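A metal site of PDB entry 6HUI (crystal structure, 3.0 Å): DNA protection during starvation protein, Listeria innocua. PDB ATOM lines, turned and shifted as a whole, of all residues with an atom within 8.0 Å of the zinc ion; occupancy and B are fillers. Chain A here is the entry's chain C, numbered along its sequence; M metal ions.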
ATOM      1  N   PHE A  12      26.651   8.255 -17.870  1.00  0.00           N
ATOM      2  CA  PHE A  12      25.726   7.156 -17.599  1.00  0.00           C
ATOM      3  C   PHE A  12      24.472   7.660 -16.881  1.00  0.00           C
ATOM      4  O   PHE A  12      23.360   7.258 -17.230  1.00  0.00           O
ATOM      5  CB  PHE A  12      26.420   6.067 -16.781  1.00  0.00           C
ATOM      6  CG  PHE A  12      25.517   4.953 -16.365  1.00  0.00           C
ATOM      7  CD1 PHE A  12      25.209   3.928 -17.243  1.00  0.00           C
ATOM      8  CD2 PHE A  12      24.955   4.922 -15.096  1.00  0.00           C
ATOM      9  CE1 PHE A  12      24.372   2.893 -16.867  1.00  0.00           C
ATOM     10  CE2 PHE A  12      24.119   3.893 -14.711  1.00  0.00           C
ATOM     11  CZ  PHE A  12      23.824   2.881 -15.598  1.00  0.00           C
ATOM     12  N   HIS A  15      22.340   9.550 -19.334  1.00  0.00           N
ATOM     13  CA  HIS A  15      21.756   8.552 -20.225  1.00  0.00           C
ATOM     14  C   HIS A  15      20.545   7.891 -19.577  1.00  0.00           C
ATOM     15  O   HIS A  15      19.487   7.738 -20.199  1.00  0.00           O
ATOM     16  CB  HIS A  15      22.822   7.511 -20.587  1.00  0.00           C
ATOM     17  CG  HIS A  15      22.415   6.586 -21.697  1.00  0.00           C
ATOM     18  ND1 HIS A  15      21.457   6.917 -22.626  1.00  0.00           N
ATOM     19  CD2 HIS A  15      22.850   5.350 -22.028  1.00  0.00           C
ATOM     20  CE1 HIS A  15      21.317   5.912 -23.474  1.00  0.00           C
ATOM     21  NE2 HIS A  15      22.154   4.950 -23.133  1.00  0.00           N
ATOM     22  N   GLN A  16      20.683   7.497 -18.305  1.00  0.00           N
ATOM     23  CA  GLN A  16      19.571   6.883 -17.588  1.00  0.00           C
ATOM     24  C   GLN A  16      18.476   7.889 -17.250  1.00  0.00           C
ATOM     25  O   GLN A  16      17.331   7.480 -17.038  1.00  0.00           O
ATOM     26  CB  GLN A  16      20.070   6.217 -16.311  1.00  0.00           C
ATOM     27  CG  GLN A  16      21.082   5.095 -16.553  1.00  0.00           C
ATOM     28  CD  GLN A  16      20.525   3.981 -17.426  1.00  0.00           C
ATOM     29  OE1 GLN A  16      19.321   3.741 -17.467  1.00  0.00           O
ATOM     30  NE2 GLN A  16      21.416   3.298 -18.137  1.00  0.00           N
ATOM     31  N   ASN A  19      16.583   7.725 -20.510  1.00  0.00           N
ATOM     32  CA  ASN A  19      15.911   6.428 -20.542  1.00  0.00           C
ATOM     33  C   ASN A  19      14.717   6.392 -19.592  1.00  0.00           C
ATOM     34  O   ASN A  19      13.671   5.836 -19.929  1.00  0.00           O
ATOM     35  CB  ASN A  19      16.902   5.322 -20.169  1.00  0.00           C
ATOM     36  CG  ASN A  19      17.996   5.160 -21.194  1.00  0.00           C
ATOM     37  OD1 ASN A  19      17.769   5.290 -22.399  1.00  0.00           O
ATOM     38  ND2 ASN A  19      19.207   4.870 -20.726  1.00  0.00           N
ATOM     39  N   ASN A  81      19.371  11.304 -26.720  1.00  0.00           N
ATOM     40  CA  ASN A  81      20.331  10.493 -25.980  1.00  0.00           C
ATOM     41  C   ASN A  81      19.760   9.205 -25.405  1.00  0.00           C
ATOM     42  O   ASN A  81      20.538   8.355 -24.948  1.00  0.00           O
ATOM     43  CB  ASN A  81      20.953  11.313 -24.831  1.00  0.00           C
ATOM     44  CG  ASN A  81      22.294  10.754 -24.373  1.00  0.00           C
ATOM     45  OD1 ASN A  81      22.499  10.509 -23.192  1.00  0.00           O
ATOM     46  ND2 ASN A  81      23.201  10.553 -25.323  1.00  0.00           N
ATOM     47  N   ALA A  82      18.443   9.022 -25.397  1.00  0.00           N
ATOM     48  CA  ALA A  82      17.876   7.824 -24.792  1.00  0.00           C
ATOM     49  C   ALA A  82      18.118   6.599 -25.666  1.00  0.00           C
ATOM     50  O   ALA A  82      18.072   6.674 -26.892  1.00  0.00           O
ATOM     51  CB  ALA A  82      16.375   8.002 -24.546  1.00  0.00           C
ATOM     52  N   SER A  83      18.383   5.468 -25.014  1.00  0.00           N
ATOM     53  CA  SER A  83      18.514   4.185 -25.694  1.00  0.00           C
ATOM     54  C   SER A  83      17.264   3.325 -25.586  1.00  0.00           C
ATOM     55  O   SER A  83      17.266   2.191 -26.074  1.00  0.00           O
ATOM     56  CB  SER A  83      19.721   3.414 -25.150  1.00  0.00           C
ATOM     57  OG  SER A  83      19.589   3.191 -23.754  1.00  0.00           O
ATOM     58  N   VAL A  84      16.207   3.824 -24.952  1.00  0.00           N
ATOM     59  CA  VAL A  84      14.936   3.110 -24.856  1.00  0.00           C
ATOM     60  C   VAL A  84      14.072   3.505 -26.038  1.00  0.00           C
ATOM     61  O   VAL A  84      13.916   4.692 -26.339  1.00  0.00           O
ATOM     62  CB  VAL A  84      14.238   3.417 -23.524  1.00  0.00           C
ATOM     63  CG1 VAL A  84      12.872   2.747 -23.467  1.00  0.00           C
ATOM     64  CG2 VAL A  84      15.098   2.976 -22.350  1.00  0.00           C
ATOM     65  N   LEU A 108      16.081  -4.105 -20.363  1.00  0.00           N
ATOM     66  CA  LEU A 108      17.060  -3.120 -20.828  1.00  0.00           C
ATOM     67  C   LEU A 108      17.639  -2.335 -19.655  1.00  0.00           C
ATOM     68  O   LEU A 108      18.859  -2.253 -19.492  1.00  0.00           O
ATOM     69  CB  LEU A 108      16.402  -2.192 -21.847  1.00  0.00           C
ATOM     70  CG  LEU A 108      17.227  -1.216 -22.696  1.00  0.00           C
ATOM     71  CD1 LEU A 108      16.456  -0.864 -23.954  1.00  0.00           C
ATOM     72  CD2 LEU A 108      17.576   0.040 -21.930  1.00  0.00           C
ATOM     73  N   LEU A 109      16.762  -1.775 -18.818  1.00  0.00           N
ATOM     74  CA  LEU A 109      17.234  -1.025 -17.661  1.00  0.00           C
ATOM     75  C   LEU A 109      17.972  -1.921 -16.668  1.00  0.00           C
ATOM     76  O   LEU A 109      18.852  -1.455 -15.942  1.00  0.00           O
ATOM     77  CB  LEU A 109      16.072  -0.312 -16.977  1.00  0.00           C
ATOM     78  CG  LEU A 109      15.404   0.797 -17.798  1.00  0.00           C
ATOM     79  CD1 LEU A 109      14.298   1.460 -16.999  1.00  0.00           C
ATOM     80  CD2 LEU A 109      16.432   1.819 -18.254  1.00  0.00           C
ATOM     81  N   GLU A 112      21.590  -2.306 -18.331  1.00  0.00           N
ATOM     82  CA  GLU A 112      22.305  -1.039 -18.263  1.00  0.00           C
ATOM     83  C   GLU A 112      22.620  -0.646 -16.819  1.00  0.00           C
ATOM     84  O   GLU A 112      23.722  -0.156 -16.531  1.00  0.00           O
ATOM     85  CB  GLU A 112      21.507   0.064 -18.952  1.00  0.00           C
ATOM     86  CG  GLU A 112      21.399  -0.108 -20.459  1.00  0.00           C
ATOM     87  CD  GLU A 112      21.279   1.221 -21.179  1.00  0.00           C
ATOM     88  OE1 GLU A 112      21.409   2.275 -20.520  1.00  0.00           O
ATOM     89  OE2 GLU A 112      21.053   1.214 -22.411  1.00  0.00           O
ATOM     90  N   GLN A 115      25.613  -2.609 -15.707  1.00  0.00           N
ATOM     91  CA  GLN A 115      26.826  -1.975 -16.214  1.00  0.00           C
ATOM     92  C   GLN A 115      27.192  -0.746 -15.399  1.00  0.00           C
ATOM     93  O   GLN A 115      28.378  -0.504 -15.127  1.00  0.00           O
ATOM     94  CB  GLN A 115      26.653  -1.613 -17.695  1.00  0.00           C
ATOM     95  CG  GLN A 115      26.519  -2.807 -18.620  1.00  0.00           C
ATOM     96  CD  GLN A 115      26.341  -2.403 -20.067  1.00  0.00           C
ATOM     97  OE1 GLN A 115      26.184  -1.225 -20.385  1.00  0.00           O
ATOM     98  NE2 GLN A 115      26.365  -3.390 -20.962  1.00  0.00           N
HETATM   99 ZN    ZN M   1      22.141   2.810 -23.591  1.00  0.00          ZN
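The backbone NH (N) of Ser 83 is in hydrogen-bond range of the side-chain amide oxygen (OD1) of Asn 19 (2.7 Å).
O of Asn 81 is in hydrogen-bond range of ND1 of His 15 (2.9 Å).
OE1 of Glu 112 lies within hydrogen-bond range of NE2 of Gln 16 (2.6 Å).
O of His 15 is in hydrogen-bond range of ND2 of Asn 19, at 2.9 Å.
ND2 of Asn 19 is in hydrogen-bond range of OE1 of Glu 112 (3.4 Å).
The zinc ion is bound by a ring nitrogen (NE2) of His 15.
OE2 of Glu 112 binds the zinc ion, 2.3 Å away.
OG of Ser 83 is bound to the zinc ion, 2.6 Å away.
The zinc ion has three donor atoms within binding distance.
Three residues have an atom within 4 Å of the zinc ion: His 15, Ser 83 and Glu 112.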
